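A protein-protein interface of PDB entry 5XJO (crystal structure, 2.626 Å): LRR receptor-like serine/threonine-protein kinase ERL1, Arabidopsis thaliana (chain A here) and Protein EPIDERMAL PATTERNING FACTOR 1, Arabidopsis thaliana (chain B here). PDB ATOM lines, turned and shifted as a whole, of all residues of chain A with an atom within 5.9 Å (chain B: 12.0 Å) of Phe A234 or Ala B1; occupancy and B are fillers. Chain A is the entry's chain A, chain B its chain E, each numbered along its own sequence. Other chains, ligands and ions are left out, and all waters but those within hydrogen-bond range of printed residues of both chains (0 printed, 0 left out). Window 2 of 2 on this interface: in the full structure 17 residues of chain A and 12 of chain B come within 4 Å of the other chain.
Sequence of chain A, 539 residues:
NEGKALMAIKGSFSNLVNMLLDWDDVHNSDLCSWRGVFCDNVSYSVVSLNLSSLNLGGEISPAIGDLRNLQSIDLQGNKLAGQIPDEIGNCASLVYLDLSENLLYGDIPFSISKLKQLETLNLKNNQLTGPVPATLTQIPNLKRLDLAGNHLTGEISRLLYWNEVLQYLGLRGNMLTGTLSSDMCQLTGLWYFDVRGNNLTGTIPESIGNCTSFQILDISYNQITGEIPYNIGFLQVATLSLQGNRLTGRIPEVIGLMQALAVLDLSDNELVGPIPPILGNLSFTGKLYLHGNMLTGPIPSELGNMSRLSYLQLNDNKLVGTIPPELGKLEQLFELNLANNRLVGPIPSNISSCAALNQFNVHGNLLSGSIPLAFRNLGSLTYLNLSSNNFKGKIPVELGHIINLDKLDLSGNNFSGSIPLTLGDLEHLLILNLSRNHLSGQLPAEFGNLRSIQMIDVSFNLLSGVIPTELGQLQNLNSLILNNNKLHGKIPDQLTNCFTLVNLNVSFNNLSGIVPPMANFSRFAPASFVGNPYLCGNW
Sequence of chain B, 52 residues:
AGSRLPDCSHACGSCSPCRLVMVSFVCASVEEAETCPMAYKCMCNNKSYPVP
The backbone carbonyl oxygen (O) of Gly B2 sits at hydrogen-bond distance from the side-chain amide nitrogen (NE2) of Gln A236.
O of Gly A233 is in hydrogen-bond range of N of Gly B2, at 3.2 Å.
The backbone NH (N) of Ser B3 is in hydrogen-bond range of the backbone carbonyl oxygen (O) of Leu A257 (2.7 Å).
The backbone carbonyl oxygen of Phe A234 sits at hydrogen-bond distance from the side-chain amide nitrogen of Gln A236.
Among the printed residues, merely in contact across the chains: Phe A234 with Ala B1 (3.4 Å), Leu A235 with Ser B3 (3.7 Å), Gln A236 with Ser B3 (3.7 Å), Leu A257 with Gly B2 (3.3 Å) and Met A258 with Ser B3 (3.0 Å).
Phe A234 touches just one residue of chain B: Ala B1.
Printed residues of chain A within 4 Å of Ala B1: Phe A234.
No residue of chain B comes within 4 Å of Gly A209.
Thr A212 touches none of the printed residues of chain B.
No residue of chain B comes within 4 Å of Tyr A230.
No residue of chain B comes within 4 Å of Asn A231.
No residue of chain B comes within 4 Å of Ile A232.
Of the printed residues of chain B, Gly A233 touches Gly B2 (3.2 Å).
Leu A235 touches just one residue of chain B: Ser B3.
Gln A236 touches just these residues of chain B: Gly B2 and Ser B3.
Of chain B, only Gly B2 and Ser B3 come within 4 Å of Leu A257.
Of the printed residues of chain A, Gly B2 touches Gly A233, Gln A236 and Leu A257.
Of the printed residues of chain B, Met A258 touches Ser B3 (3.0 Å).
Printed residues of chain A within 4 Å of Ser B3: Leu A235 (3.7 Å), Gln A236 (3.7 Å), Leu A257 (2.7 Å) and Met A258 (3.0 Å).
Pro B52 touches none of the printed residues of chain A.
Of the 13 printed residues of chain A, 6 touch a printed residue of chain B.
Printed residues of chain A that touch a printed residue of chain B: Gly A233, Phe A234, Leu A235, Gln A236, Leu A257 and Met A258.
Hydrophobic or aromatic side chains of chain A within 4 Å of the printed part of chain B: Phe A234, Leu A257 and Met A258.
Printed residues of chain B that touch a printed residue of chain A: Ala B1, Gly B2 and Ser B3.
Hydrophobic or aromatic side chains of chain B that line the printed part of chain A: Ala B1.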
ATOM      1  N   GLY A 209      19.003 -20.076 -12.856  1.00  0.00           N
ATOM      2  CA  GLY A 209      17.796 -19.391 -13.275  1.00  0.00           C
ATOM      3  C   GLY A 209      16.527 -20.196 -13.082  1.00  0.00           C
ATOM      4  O   GLY A 209      15.434 -19.619 -13.128  1.00  0.00           O
ATOM      5  N   ASN A 210      16.649 -21.515 -12.854  1.00  0.00           N
ATOM      6  CA  ASN A 210      15.505 -22.397 -12.665  1.00  0.00           C
ATOM      7  C   ASN A 210      14.930 -22.354 -11.253  1.00  0.00           C
ATOM      8  O   ASN A 210      13.868 -22.946 -11.025  1.00  0.00           O
ATOM      9  CB  ASN A 210      15.898 -23.840 -13.022  1.00  0.00           C
ATOM     10  CG  ASN A 210      16.051 -24.066 -14.537  1.00  0.00           C
ATOM     11  OD1 ASN A 210      15.075 -23.959 -15.293  1.00  0.00           O
ATOM     12  ND2 ASN A 210      17.280 -24.397 -14.982  1.00  0.00           N
ATOM     13  N   THR A 212      13.219 -20.263  -9.503  1.00  0.00           N
ATOM     14  CA  THR A 212      12.352 -19.088  -9.473  1.00  0.00           C
ATOM     15  C   THR A 212      11.482 -18.982  -8.219  1.00  0.00           C
ATOM     16  O   THR A 212      10.761 -17.993  -8.102  1.00  0.00           O
ATOM     17  CB  THR A 212      11.438 -19.049 -10.723  1.00  0.00           C
ATOM     18  OG1 THR A 212      10.446 -20.086 -10.637  1.00  0.00           O
ATOM     19  CG2 THR A 212      12.242 -19.261 -11.991  1.00  0.00           C
ATOM     20  N   TYR A 230      24.608 -15.405 -16.707  1.00  0.00           N
ATOM     21  CA  TYR A 230      23.471 -14.681 -17.262  1.00  0.00           C
ATOM     22  C   TYR A 230      22.157 -15.146 -16.643  1.00  0.00           C
ATOM     23  O   TYR A 230      21.258 -14.331 -16.396  1.00  0.00           O
ATOM     24  CB  TYR A 230      23.428 -14.842 -18.779  1.00  0.00           C
ATOM     25  CG  TYR A 230      22.204 -14.194 -19.425  1.00  0.00           C
ATOM     26  CD1 TYR A 230      22.113 -12.803 -19.578  1.00  0.00           C
ATOM     27  CD2 TYR A 230      21.145 -14.974 -19.885  1.00  0.00           C
ATOM     28  CE1 TYR A 230      21.003 -12.217 -20.160  1.00  0.00           C
ATOM     29  CE2 TYR A 230      20.026 -14.394 -20.473  1.00  0.00           C
ATOM     30  CZ  TYR A 230      19.960 -13.016 -20.612  1.00  0.00           C
ATOM     31  OH  TYR A 230      18.845 -12.451 -21.208  1.00  0.00           O
ATOM     32  N   ASN A 231      22.039 -16.449 -16.345  1.00  0.00           N
ATOM     33  CA  ASN A 231      20.758 -16.943 -15.842  1.00  0.00           C
ATOM     34  C   ASN A 231      20.473 -16.548 -14.394  1.00  0.00           C
ATOM     35  O   ASN A 231      19.352 -16.819 -13.920  1.00  0.00           O
ATOM     36  CB  ASN A 231      20.651 -18.471 -16.003  1.00  0.00           C
ATOM     37  CG  ASN A 231      20.397 -18.892 -17.461  1.00  0.00           C
ATOM     38  OD1 ASN A 231      19.922 -18.099 -18.276  1.00  0.00           O
ATOM     39  ND2 ASN A 231      20.659 -20.148 -17.770  1.00  0.00           N
ATOM     40  N   ILE A 232      21.401 -15.857 -13.716  1.00  0.00           N
ATOM     41  CA  ILE A 232      21.054 -15.127 -12.500  1.00  0.00           C
ATOM     42  C   ILE A 232      19.880 -14.186 -12.776  1.00  0.00           C
ATOM     43  O   ILE A 232      19.106 -13.852 -11.871  1.00  0.00           O
ATOM     44  CB  ILE A 232      22.291 -14.363 -11.952  1.00  0.00           C
ATOM     45  CG1 ILE A 232      22.150 -14.103 -10.457  1.00  0.00           C
ATOM     46  CG2 ILE A 232      22.483 -13.015 -12.646  1.00  0.00           C
ATOM     47  CD1 ILE A 232      22.288 -15.332  -9.627  1.00  0.00           C
ATOM     48  N   GLY A 233      19.719 -13.760 -14.026  1.00  0.00           N
ATOM     49  CA  GLY A 233      18.654 -12.843 -14.381  1.00  0.00           C
ATOM     50  C   GLY A 233      17.274 -13.429 -14.278  1.00  0.00           C
ATOM     51  O   GLY A 233      16.298 -12.666 -14.336  1.00  0.00           O
ATOM     52  N   PHE A 234      17.157 -14.757 -14.117  1.00  0.00           N
ATOM     53  CA  PHE A 234      15.820 -15.331 -14.098  1.00  0.00           C
ATOM     54  C   PHE A 234      15.263 -15.460 -12.703  1.00  0.00           C
ATOM     55  O   PHE A 234      14.048 -15.663 -12.557  1.00  0.00           O
ATOM     56  CB  PHE A 234      15.791 -16.693 -14.793  1.00  0.00           C
ATOM     57  CG  PHE A 234      15.895 -16.610 -16.281  1.00  0.00           C
ATOM     58  CD1 PHE A 234      17.111 -16.332 -16.894  1.00  0.00           C
ATOM     59  CD2 PHE A 234      14.781 -16.830 -17.072  1.00  0.00           C
ATOM     60  CE1 PHE A 234      17.216 -16.265 -18.273  1.00  0.00           C
ATOM     61  CE2 PHE A 234      14.871 -16.772 -18.457  1.00  0.00           C
ATOM     62  CZ  PHE A 234      16.090 -16.477 -19.060  1.00  0.00           C
ATOM     63  N   LEU A 235      16.098 -15.325 -11.683  1.00  0.00           N
ATOM     64  CA  LEU A 235      15.598 -15.473 -10.326  1.00  0.00           C
ATOM     65  C   LEU A 235      14.577 -14.395 -10.007  1.00  0.00           C
ATOM     66  O   LEU A 235      14.622 -13.283 -10.549  1.00  0.00           O
ATOM     67  CB  LEU A 235      16.742 -15.444  -9.307  1.00  0.00           C
ATOM     68  CG  LEU A 235      17.849 -16.477  -9.446  1.00  0.00           C
ATOM     69  CD1 LEU A 235      18.983 -16.153  -8.500  1.00  0.00           C
ATOM     70  CD2 LEU A 235      17.256 -17.881  -9.193  1.00  0.00           C
ATOM     71  N   GLN A 236      13.627 -14.746  -9.139  1.00  0.00           N
ATOM     72  CA  GLN A 236      12.632 -13.825  -8.611  1.00  0.00           C
ATOM     73  C   GLN A 236      12.897 -13.489  -7.156  1.00  0.00           C
ATOM     74  O   GLN A 236      11.968 -13.124  -6.428  1.00  0.00           O
ATOM     75  CB  GLN A 236      11.240 -14.410  -8.784  1.00  0.00           C
ATOM     76  CG  GLN A 236      11.082 -15.077 -10.135  1.00  0.00           C
ATOM     77  CD  GLN A 236      10.710 -14.077 -11.199  1.00  0.00           C
ATOM     78  OE1 GLN A 236       9.657 -13.451 -11.098  1.00  0.00           O
ATOM     79  NE2 GLN A 236      11.601 -13.854 -12.176  1.00  0.00           N
ATOM     80  N   VAL A 254      22.019  -8.222 -17.215  1.00  0.00           N
ATOM     81  CA  VAL A 254      20.709  -8.804 -16.957  1.00  0.00           C
ATOM     82  C   VAL A 254      20.248  -8.515 -15.537  1.00  0.00           C
ATOM     83  O   VAL A 254      19.050  -8.601 -15.247  1.00  0.00           O
ATOM     84  CB  VAL A 254      20.722 -10.324 -17.221  1.00  0.00           C
ATOM     85  CG1 VAL A 254      21.493 -11.063 -16.117  1.00  0.00           C
ATOM     86  CG2 VAL A 254      19.289 -10.871 -17.370  1.00  0.00           C
ATOM     87  N   LEU A 257      17.444  -6.155 -15.129  1.00  0.00           N
ATOM     88  CA  LEU A 257      16.071  -6.566 -15.393  1.00  0.00           C
ATOM     89  C   LEU A 257      15.403  -7.191 -14.173  1.00  0.00           C
ATOM     90  O   LEU A 257      14.227  -7.585 -14.253  1.00  0.00           O
ATOM     91  CB  LEU A 257      16.045  -7.546 -16.580  1.00  0.00           C
ATOM     92  CG  LEU A 257      16.823  -7.019 -17.795  1.00  0.00           C
ATOM     93  CD1 LEU A 257      17.035  -8.092 -18.844  1.00  0.00           C
ATOM     94  CD2 LEU A 257      16.121  -5.800 -18.397  1.00  0.00           C
ATOM     95  N   MET A 258      16.111  -7.254 -13.038  1.00  0.00           N
ATOM     96  CA  MET A 258      15.611  -7.938 -11.845  1.00  0.00           C
ATOM     97  C   MET A 258      14.946  -6.930 -10.911  1.00  0.00           C
ATOM     98  O   MET A 258      15.382  -6.682  -9.787  1.00  0.00           O
ATOM     99  CB  MET A 258      16.739  -8.689 -11.143  1.00  0.00           C
ATOM    100  CG  MET A 258      17.448  -9.724 -12.006  1.00  0.00           C
ATOM    101  SD  MET A 258      18.937 -10.394 -11.231  1.00  0.00           S
ATOM    102  CE  MET A 258      18.261 -11.057  -9.705  1.00  0.00           C
ATOM    103  N   ALA B   1      15.832 -12.939 -18.431  1.00  0.00           N
ATOM    104  CA  ALA B   1      14.499 -12.535 -18.855  1.00  0.00           C
ATOM    105  C   ALA B   1      14.025 -11.412 -17.940  1.00  0.00           C
ATOM    106  O   ALA B   1      13.409 -10.437 -18.391  1.00  0.00           O
ATOM    107  CB  ALA B   1      13.532 -13.718 -18.830  1.00  0.00           C
ATOM    108  N   GLY B   2      14.388 -11.555 -16.678  1.00  0.00           N
ATOM    109  CA  GLY B   2      14.121 -10.593 -15.636  1.00  0.00           C
ATOM    110  C   GLY B   2      13.162 -10.891 -14.509  1.00  0.00           C
ATOM    111  O   GLY B   2      12.753 -12.000 -14.299  1.00  0.00           O
ATOM    112  N   SER B   3      12.830  -9.848 -13.762  1.00  0.00           N
ATOM    113  CA  SER B   3      11.868  -9.921 -12.673  1.00  0.00           C
ATOM    114  C   SER B   3      11.058  -8.640 -12.544  1.00  0.00           C
ATOM    115  O   SER B   3      11.336  -7.665 -13.148  1.00  0.00           O
ATOM    116  CB  SER B   3      12.492 -10.360 -11.338  1.00  0.00           C
ATOM    117  OG  SER B   3      13.254  -9.390 -10.679  1.00  0.00           O
ATOM    118  N   ARG B   4      10.004  -8.690 -11.782  1.00  0.00           N
ATOM    119  CA  ARG B   4       9.176  -7.540 -11.571  1.00  0.00           C
ATOM    120  C   ARG B   4       8.727  -7.532 -10.152  1.00  0.00           C
ATOM    121  O   ARG B   4       8.754  -8.533  -9.488  1.00  0.00           O
ATOM    122  CB  ARG B   4       7.917  -7.634 -12.424  1.00  0.00           C
ATOM    123  CG  ARG B   4       8.119  -7.548 -13.923  1.00  0.00           C
ATOM    124  CD  ARG B   4       6.791  -7.603 -14.658  1.00  0.00           C
ATOM    125  NE  ARG B   4       6.970  -7.592 -16.105  1.00  0.00           N
ATOM    126  CZ  ARG B   4       5.988  -7.748 -16.985  1.00  0.00           C
ATOM    127  NH1 ARG B   4       4.743  -7.928 -16.580  1.00  0.00           N
ATOM    128  NH2 ARG B   4       6.244  -7.709 -18.280  1.00  0.00           N
ATOM    129  N   LEU B   5       8.259  -6.395  -9.699  1.00  0.00           N
ATOM    130  CA  LEU B   5       7.738  -6.270  -8.370  1.00  0.00           C
ATOM    131  C   LEU B   5       6.396  -6.966  -8.274  1.00  0.00           C
ATOM    132  O   LEU B   5       5.546  -6.694  -9.053  1.00  0.00           O
ATOM    133  CB  LEU B   5       7.586  -4.800  -8.099  1.00  0.00           C
ATOM    134  CG  LEU B   5       7.035  -4.395  -6.765  1.00  0.00           C
ATOM    135  CD1 LEU B   5       8.063  -4.751  -5.737  1.00  0.00           C
ATOM    136  CD2 LEU B   5       6.769  -2.909  -6.766  1.00  0.00           C
ATOM    137  N   PRO B   6       6.194  -7.872  -7.314  1.00  0.00           N
ATOM    138  CA  PRO B   6       4.903  -8.580  -7.248  1.00  0.00           C
ATOM    139  C   PRO B   6       3.731  -7.624  -7.120  1.00  0.00           C
ATOM    140  O   PRO B   6       3.761  -6.664  -6.355  1.00  0.00           O
ATOM    141  CB  PRO B   6       5.046  -9.478  -6.009  1.00  0.00           C
ATOM    142  CG  PRO B   6       6.464  -9.742  -5.886  1.00  0.00           C
ATOM    143  CD  PRO B   6       7.224  -8.581  -6.531  1.00  0.00           C
ATOM    144  N   PRO B  52       2.204 -13.214  -5.566  1.00  0.00           N
ATOM    145  CA  PRO B  52       2.122 -14.098  -6.753  1.00  0.00           C
ATOM    146  C   PRO B  52       3.492 -14.552  -7.223  1.00  0.00           C
ATOM    147  O   PRO B  52       3.779 -15.729  -7.017  1.00  0.00           O
ATOM    148  CB  PRO B  52       1.447 -13.231  -7.825  1.00  0.00           C
ATOM    149  CG  PRO B  52       0.667 -12.229  -7.052  1.00  0.00           C
ATOM    150  CD  PRO B  52       1.344 -12.026  -5.702  1.00  0.00           C
